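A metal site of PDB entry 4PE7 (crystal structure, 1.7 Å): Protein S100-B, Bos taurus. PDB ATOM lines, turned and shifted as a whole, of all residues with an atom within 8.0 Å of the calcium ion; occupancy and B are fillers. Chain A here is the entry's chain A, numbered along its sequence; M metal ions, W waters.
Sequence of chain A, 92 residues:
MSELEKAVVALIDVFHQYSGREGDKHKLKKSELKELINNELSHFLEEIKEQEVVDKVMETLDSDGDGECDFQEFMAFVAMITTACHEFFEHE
The backbone NH of Lys 29 lies close to the side-chain carboxylate of Glu 32, at 2.9 Å. The side-chain carboxylate (OE2) of Glu 32 lies close to the backbone NH (N) of Arg 21, at 3.4 Å. The side-chain carboxylate (OD1) of Asp 24 is in hydrogen-bond range of the backbone NH (N) of His 26 (2.9 Å). The side-chain carboxylate of Glu 22 lies within salt-bridge range of the side-chain amino group of Lys 29 (3.1 Å). OD2 of Asp 24 lies within salt-bridge range of NZ of Lys 27. The side-chain hydroxyl of Ser 19 is in hydrogen-bond range of the backbone carbonyl oxygen of Phe 15, 2.7 Å away. The side-chain hydroxyl of Ser 19 lies within hydrogen-bond range of the backbone carbonyl oxygen of Lys 25 (2.9 Å). The backbone carbonyl oxygen (O) of His 16 sits at hydrogen-bond distance from the side-chain hydroxyl (OG) of Ser 19 (3.5 Å).
Water W1 binds the calcium ion, 2.3 Å away. The backbone carbonyl oxygen (O) of Ser 19 is bound to the calcium ion (2.3 Å). O of Asp 24 is bound to the calcium ion (2.4 Å). O of Glu 22 is bound to the calcium ion (2.4 Å). The calcium ion is bound by O of Lys 27 (2.4 Å). OE1 of Glu 32 is bound to the calcium ion (2.4 Å). The calcium ion is bound by OE2 of Glu 32.
Five residues have an atom within 4 Å of the calcium ion: Ser 19, Glu 22, Asp 24, Lys 27 and Glu 32.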
ATOM      1  N   PHE A  15     -11.711  18.886 -15.207  1.00  0.00           N
ATOM      2  CA  PHE A  15     -12.830  18.529 -14.342  1.00  0.00           C
ATOM      3  C   PHE A  15     -13.996  19.504 -14.535  1.00  0.00           C
ATOM      4  O   PHE A  15     -15.149  19.094 -14.591  1.00  0.00           O
ATOM      5  CB  PHE A  15     -12.425  18.476 -12.866  1.00  0.00           C
ATOM      6  CG  PHE A  15     -13.539  18.039 -11.950  1.00  0.00           C
ATOM      7  CD1 PHE A  15     -13.771  16.690 -11.708  1.00  0.00           C
ATOM      8  CD2 PHE A  15     -14.383  18.984 -11.365  1.00  0.00           C
ATOM      9  CE1 PHE A  15     -14.793  16.269 -10.871  1.00  0.00           C
ATOM     10  CE2 PHE A  15     -15.412  18.584 -10.531  1.00  0.00           C
ATOM     11  CZ  PHE A  15     -15.631  17.231 -10.286  1.00  0.00           C
ATOM     12  N   HIS A  16     -13.677  20.796 -14.634  1.00  0.00           N
ATOM     13  CA  HIS A  16     -14.687  21.834 -14.819  1.00  0.00           C
ATOM     14  C   HIS A  16     -15.471  21.587 -16.097  1.00  0.00           C
ATOM     15  O   HIS A  16     -16.711  21.641 -16.101  1.00  0.00           O
ATOM     16  CB  HIS A  16     -14.001  23.198 -14.892  1.00  0.00           C
ATOM     17  CG  HIS A  16     -14.940  24.332 -15.141  1.00  0.00           C
ATOM     18  ND1 HIS A  16     -15.641  24.953 -14.127  1.00  0.00           N
ATOM     19  CD2 HIS A  16     -15.286  24.983 -16.286  1.00  0.00           C
ATOM     20  CE1 HIS A  16     -16.391  25.920 -14.640  1.00  0.00           C
ATOM     21  NE2 HIS A  16     -16.191  25.949 -15.941  1.00  0.00           N
ATOM     22  N   GLN A  17     -14.746  21.323 -17.181  1.00  0.00           N
ATOM     23  CA  GLN A  17     -15.352  21.119 -18.493  1.00  0.00           C
ATOM     24  C   GLN A  17     -16.390  20.007 -18.478  1.00  0.00           C
ATOM     25  O   GLN A  17     -17.517  20.182 -18.954  1.00  0.00           O
ATOM     26  CB  GLN A  17     -14.278  20.828 -19.554  1.00  0.00           C
ATOM     27  CG  GLN A  17     -13.318  21.985 -19.801  1.00  0.00           C
ATOM     28  CD  GLN A  17     -11.991  21.534 -20.406  1.00  0.00           C
ATOM     29  OE1 GLN A  17     -11.827  20.372 -20.814  1.00  0.00           O
ATOM     30  NE2 GLN A  17     -11.014  22.453 -20.449  1.00  0.00           N
ATOM     31  N   TYR A  18     -16.008  18.861 -17.910  1.00  0.00           N
ATOM     32  CA  TYR A  18     -16.876  17.680 -17.877  1.00  0.00           C
ATOM     33  C   TYR A  18     -17.957  17.693 -16.789  1.00  0.00           C
ATOM     34  O   TYR A  18     -19.085  17.270 -17.039  1.00  0.00           O
ATOM     35  CB  TYR A  18     -16.033  16.384 -17.845  1.00  0.00           C
ATOM     36  CG  TYR A  18     -15.418  16.120 -19.199  1.00  0.00           C
ATOM     37  CD1 TYR A  18     -14.196  16.686 -19.549  1.00  0.00           C
ATOM     38  CD2 TYR A  18     -16.094  15.350 -20.155  1.00  0.00           C
ATOM     39  CE1 TYR A  18     -13.653  16.491 -20.814  1.00  0.00           C
ATOM     40  CE2 TYR A  18     -15.555  15.150 -21.412  1.00  0.00           C
ATOM     41  CZ  TYR A  18     -14.341  15.726 -21.735  1.00  0.00           C
ATOM     42  OH  TYR A  18     -13.796  15.525 -22.979  1.00  0.00           O
ATOM     43  N   SER A  19     -17.635  18.204 -15.601  1.00  0.00           N
ATOM     44  CA  SER A  19     -18.599  18.190 -14.500  1.00  0.00           C
ATOM     45  C   SER A  19     -19.759  19.142 -14.790  1.00  0.00           C
ATOM     46  O   SER A  19     -20.885  18.906 -14.343  1.00  0.00           O
ATOM     47  CB  SER A  19     -17.932  18.556 -13.180  1.00  0.00           C
ATOM     48  OG  SER A  19     -17.390  19.872 -13.210  1.00  0.00           O
ATOM     49  N   GLY A  20     -19.487  20.184 -15.567  1.00  0.00           N
ATOM     50  CA  GLY A  20     -20.470  21.236 -15.807  1.00  0.00           C
ATOM     51  C   GLY A  20     -21.483  20.931 -16.897  1.00  0.00           C
ATOM     52  O   GLY A  20     -22.377  21.746 -17.150  1.00  0.00           O
ATOM     53  N   ARG A  21     -21.365  19.773 -17.538  1.00  0.00           N
ATOM     54  CA  ARG A  21     -22.272  19.444 -18.640  1.00  0.00           C
ATOM     55  C   ARG A  21     -23.724  19.268 -18.198  1.00  0.00           C
ATOM     56  O   ARG A  21     -24.646  19.840 -18.802  1.00  0.00           O
ATOM     57  CB  ARG A  21     -21.776  18.198 -19.383  1.00  0.00           C
ATOM     58  CG  ARG A  21     -20.444  18.414 -20.086  1.00  0.00           C
ATOM     59  CD  ARG A  21     -19.940  17.149 -20.727  1.00  0.00           C
ATOM     60  NE  ARG A  21     -18.857  17.419 -21.657  1.00  0.00           N
ATOM     61  CZ  ARG A  21     -18.467  16.570 -22.613  1.00  0.00           C
ATOM     62  NH1 ARG A  21     -19.069  15.405 -22.757  1.00  0.00           N
ATOM     63  NH2 ARG A  21     -17.476  16.911 -23.424  1.00  0.00           N
ATOM     64  N   GLU A  22     -23.923  18.477 -17.147  1.00  0.00           N
ATOM     65  CA  GLU A  22     -25.265  18.105 -16.723  1.00  0.00           C
ATOM     66  C   GLU A  22     -25.385  18.035 -15.199  1.00  0.00           C
ATOM     67  O   GLU A  22     -24.400  17.768 -14.488  1.00  0.00           O
ATOM     68  CB  GLU A  22     -25.656  16.754 -17.318  1.00  0.00           C
ATOM     69  CG  GLU A  22     -25.766  16.744 -18.838  1.00  0.00           C
ATOM     70  CD  GLU A  22     -26.055  15.359 -19.392  1.00  0.00           C
ATOM     71  OE1 GLU A  22     -26.720  14.564 -18.703  1.00  0.00           O
ATOM     72  OE2 GLU A  22     -25.599  15.081 -20.519  1.00  0.00           O
ATOM     73  N   GLY A  23     -26.601  18.275 -14.705  1.00  0.00           N
ATOM     74  CA  GLY A  23     -26.901  18.130 -13.303  1.00  0.00           C
ATOM     75  C   GLY A  23     -26.033  18.991 -12.418  1.00  0.00           C
ATOM     76  O   GLY A  23     -25.813  20.178 -12.689  1.00  0.00           O
ATOM     77  N   ASP A  24     -25.533  18.390 -11.335  1.00  0.00           N
ATOM     78  CA  ASP A  24     -24.583  19.041 -10.451  1.00  0.00           C
ATOM     79  C   ASP A  24     -23.369  19.452 -11.286  1.00  0.00           C
ATOM     80  O   ASP A  24     -22.706  18.610 -11.898  1.00  0.00           O
ATOM     81  CB  ASP A  24     -24.192  18.050  -9.359  1.00  0.00           C
ATOM     82  CG  ASP A  24     -23.425  18.702  -8.222  1.00  0.00           C
ATOM     83  OD1 ASP A  24     -22.679  19.675  -8.459  1.00  0.00           O
ATOM     84  OD2 ASP A  24     -23.580  18.220  -7.079  1.00  0.00           O
ATOM     85  N   LYS A  25     -23.097  20.749 -11.314  1.00  0.00           N
ATOM     86  CA  LYS A  25     -22.007  21.270 -12.127  1.00  0.00           C
ATOM     87  C   LYS A  25     -20.644  21.043 -11.489  1.00  0.00           C
ATOM     88  O   LYS A  25     -19.619  21.371 -12.100  1.00  0.00           O
ATOM     89  CB  LYS A  25     -22.203  22.762 -12.410  1.00  0.00           C
ATOM     90  CG  LYS A  25     -23.392  23.051 -13.315  1.00  0.00           C
ATOM     91  CD  LYS A  25     -23.562  24.534 -13.594  1.00  0.00           C
ATOM     92  CE  LYS A  25     -24.617  24.762 -14.671  1.00  0.00           C
ATOM     93  NZ  LYS A  25     -24.232  24.132 -15.960  1.00  0.00           N
ATOM     94  N   HIS A  26     -20.624  20.480 -10.285  1.00  0.00           N
ATOM     95  CA  HIS A  26     -19.353  20.224  -9.599  1.00  0.00           C
ATOM     96  C   HIS A  26     -19.089  18.739  -9.348  1.00  0.00           C
ATOM     97  O   HIS A  26     -18.159  18.381  -8.626  1.00  0.00           O
ATOM     98  CB  HIS A  26     -19.258  21.034  -8.300  1.00  0.00           C
ATOM     99  CG  HIS A  26     -19.399  22.515  -8.522  1.00  0.00           C
ATOM    100  ND1 HIS A  26     -18.527  23.232  -9.307  1.00  0.00           N
ATOM    101  CD2 HIS A  26     -20.330  23.395  -8.091  1.00  0.00           C
ATOM    102  CE1 HIS A  26     -18.904  24.499  -9.338  1.00  0.00           C
ATOM    103  NE2 HIS A  26     -19.993  24.622  -8.601  1.00  0.00           N
ATOM    104  N   LYS A  27     -19.902  17.896  -9.971  1.00  0.00           N
ATOM    105  CA  LYS A  27     -19.660  16.456  -9.920  1.00  0.00           C
ATOM    106  C   LYS A  27     -19.810  15.852 -11.298  1.00  0.00           C
ATOM    107  O   LYS A  27     -20.551  16.382 -12.144  1.00  0.00           O
ATOM    108  CB  LYS A  27     -20.637  15.772  -8.970  1.00  0.00           C
ATOM    109  CG  LYS A  27     -20.544  16.220  -7.511  1.00  0.00           C
ATOM    110  CD  LYS A  27     -21.540  15.443  -6.684  1.00  0.00           C
ATOM    111  CE  LYS A  27     -21.589  15.914  -5.237  1.00  0.00           C
ATOM    112  NZ  LYS A  27     -22.828  15.366  -4.590  1.00  0.00           N
ATOM    113  N   LEU A  28     -19.121  14.730 -11.508  1.00  0.00           N
ATOM    114  CA  LEU A  28     -19.225  13.950 -12.731  1.00  0.00           C
ATOM    115  C   LEU A  28     -20.237  12.840 -12.536  1.00  0.00           C
ATOM    116  O   LEU A  28     -20.037  11.989 -11.661  1.00  0.00           O
ATOM    117  CB  LEU A  28     -17.865  13.318 -13.056  1.00  0.00           C
ATOM    118  CG  LEU A  28     -16.705  14.261 -13.312  1.00  0.00           C
ATOM    119  CD1 LEU A  28     -15.377  13.499 -13.166  1.00  0.00           C
ATOM    120  CD2 LEU A  28     -16.800  14.852 -14.697  1.00  0.00           C
ATOM    121  N   LYS A  29     -21.303  12.829 -13.322  1.00  0.00           N
ATOM    122  CA  LYS A  29     -22.187  11.663 -13.395  1.00  0.00           C
ATOM    123  C   LYS A  29     -21.562  10.625 -14.333  1.00  0.00           C
ATOM    124  O   LYS A  29     -20.518  10.885 -14.929  1.00  0.00           O
ATOM    125  CB  LYS A  29     -23.581  12.067 -13.889  1.00  0.00           C
ATOM    126  CG  LYS A  29     -23.618  12.509 -15.343  1.00  0.00           C
ATOM    127  CD  LYS A  29     -24.874  13.304 -15.688  1.00  0.00           C
ATOM    128  CE  LYS A  29     -26.129  12.474 -15.605  1.00  0.00           C
ATOM    129  NZ  LYS A  29     -27.323  13.334 -15.914  1.00  0.00           N
ATOM    130  N   LYS A  30     -22.209   9.480 -14.480  1.00  0.00           N
ATOM    131  CA  LYS A  30     -21.651   8.407 -15.305  1.00  0.00           C
ATOM    132  C   LYS A  30     -21.299   8.857 -16.725  1.00  0.00           C
ATOM    133  O   LYS A  30     -20.201   8.585 -17.208  1.00  0.00           O
ATOM    134  CB  LYS A  30     -22.592   7.211 -15.367  1.00  0.00           C
ATOM    135  CG  LYS A  30     -22.552   6.313 -14.138  1.00  0.00           C
ATOM    136  CD  LYS A  30     -23.666   5.272 -14.254  1.00  0.00           C
ATOM    137  CE  LYS A  30     -23.629   4.250 -13.136  1.00  0.00           C
ATOM    138  NZ  LYS A  30     -24.725   3.243 -13.347  1.00  0.00           N
ATOM    139  N   SER A  31     -22.226   9.546 -17.384  1.00  0.00           N
ATOM    140  CA  SER A  31     -21.989   9.957 -18.771  1.00  0.00           C
ATOM    141  C   SER A  31     -20.826  10.927 -18.887  1.00  0.00           C
ATOM    142  O   SER A  31     -20.030  10.848 -19.835  1.00  0.00           O
ATOM    143  CB  SER A  31     -23.264  10.550 -19.390  1.00  0.00           C
ATOM    144  OG  SER A  31     -23.665  11.714 -18.699  1.00  0.00           O
ATOM    145  N   GLU A  32     -20.699  11.839 -17.918  1.00  0.00           N
ATOM    146  CA  GLU A  32     -19.621  12.828 -17.931  1.00  0.00           C
ATOM    147  C   GLU A  32     -18.251  12.187 -17.697  1.00  0.00           C
ATOM    148  O   GLU A  32     -17.263  12.569 -18.349  1.00  0.00           O
ATOM    149  CB  GLU A  32     -19.875  13.914 -16.894  1.00  0.00           C
ATOM    150  CG  GLU A  32     -21.077  14.819 -17.202  1.00  0.00           C
ATOM    151  CD  GLU A  32     -21.501  15.673 -16.011  1.00  0.00           C
ATOM    152  OE1 GLU A  32     -21.235  15.281 -14.861  1.00  0.00           O
ATOM    153  OE2 GLU A  32     -22.072  16.751 -16.225  1.00  0.00           O
ATOM    154  N   LEU A  33     -18.196  11.252 -16.752  1.00  0.00           N
ATOM    155  CA  LEU A  33     -16.967  10.539 -16.441  1.00  0.00           C
ATOM    156  C   LEU A  33     -16.538   9.677 -17.635  1.00  0.00           C
ATOM    157  O   LEU A  33     -15.354   9.604 -17.954  1.00  0.00           O
ATOM    158  CB  LEU A  33     -17.209   9.656 -15.216  1.00  0.00           C
ATOM    159  CG  LEU A  33     -16.074   8.722 -14.778  1.00  0.00           C
ATOM    160  CD1 LEU A  33     -14.890   9.556 -14.383  1.00  0.00           C
ATOM    161  CD2 LEU A  33     -16.512   7.830 -13.615  1.00  0.00           C
ATOM    162  N   GLU A  68     -21.965   9.754  -7.882  1.00  0.00           N
ATOM    163  CA  GLU A  68     -21.246  10.661  -8.778  1.00  0.00           C
ATOM    164  C   GLU A  68     -19.807  10.794  -8.336  1.00  0.00           C
ATOM    165  O   GLU A  68     -19.471  10.396  -7.213  1.00  0.00           O
ATOM    166  CB  GLU A  68     -21.920  12.051  -8.865  1.00  0.00           C
ATOM    167  CG  GLU A  68     -23.375  12.037  -9.387  1.00  0.00           C
ATOM    168  CD  GLU A  68     -23.812  13.352 -10.007  1.00  0.00           C
ATOM    169  OE1 GLU A  68     -22.948  14.123 -10.471  1.00  0.00           O
ATOM    170  OE2 GLU A  68     -25.032  13.606 -10.043  1.00  0.00           O
ATOM    171  N   CYS A  69     -18.968  11.331  -9.204  1.00  0.00           N
ATOM    172  CA  CYS A  69     -17.561  11.528  -8.856  1.00  0.00           C
ATOM    173  C   CYS A  69     -17.292  13.003  -8.620  1.00  0.00           C
ATOM    174  O   CYS A  69     -17.368  13.818  -9.547  1.00  0.00           O
ATOM    175  CB  CYS A  69     -16.653  11.018  -9.999  1.00  0.00           C
ATOM    176  SG  CYS A  69     -14.870  11.118  -9.663  1.00  0.00           S
HETATM  177 CA    CA M   1     -22.256  17.135 -13.683  1.00  0.00          CA
HETATM  178  O   HOH W   1     -23.557  15.559 -12.566  1.00  0.00           O
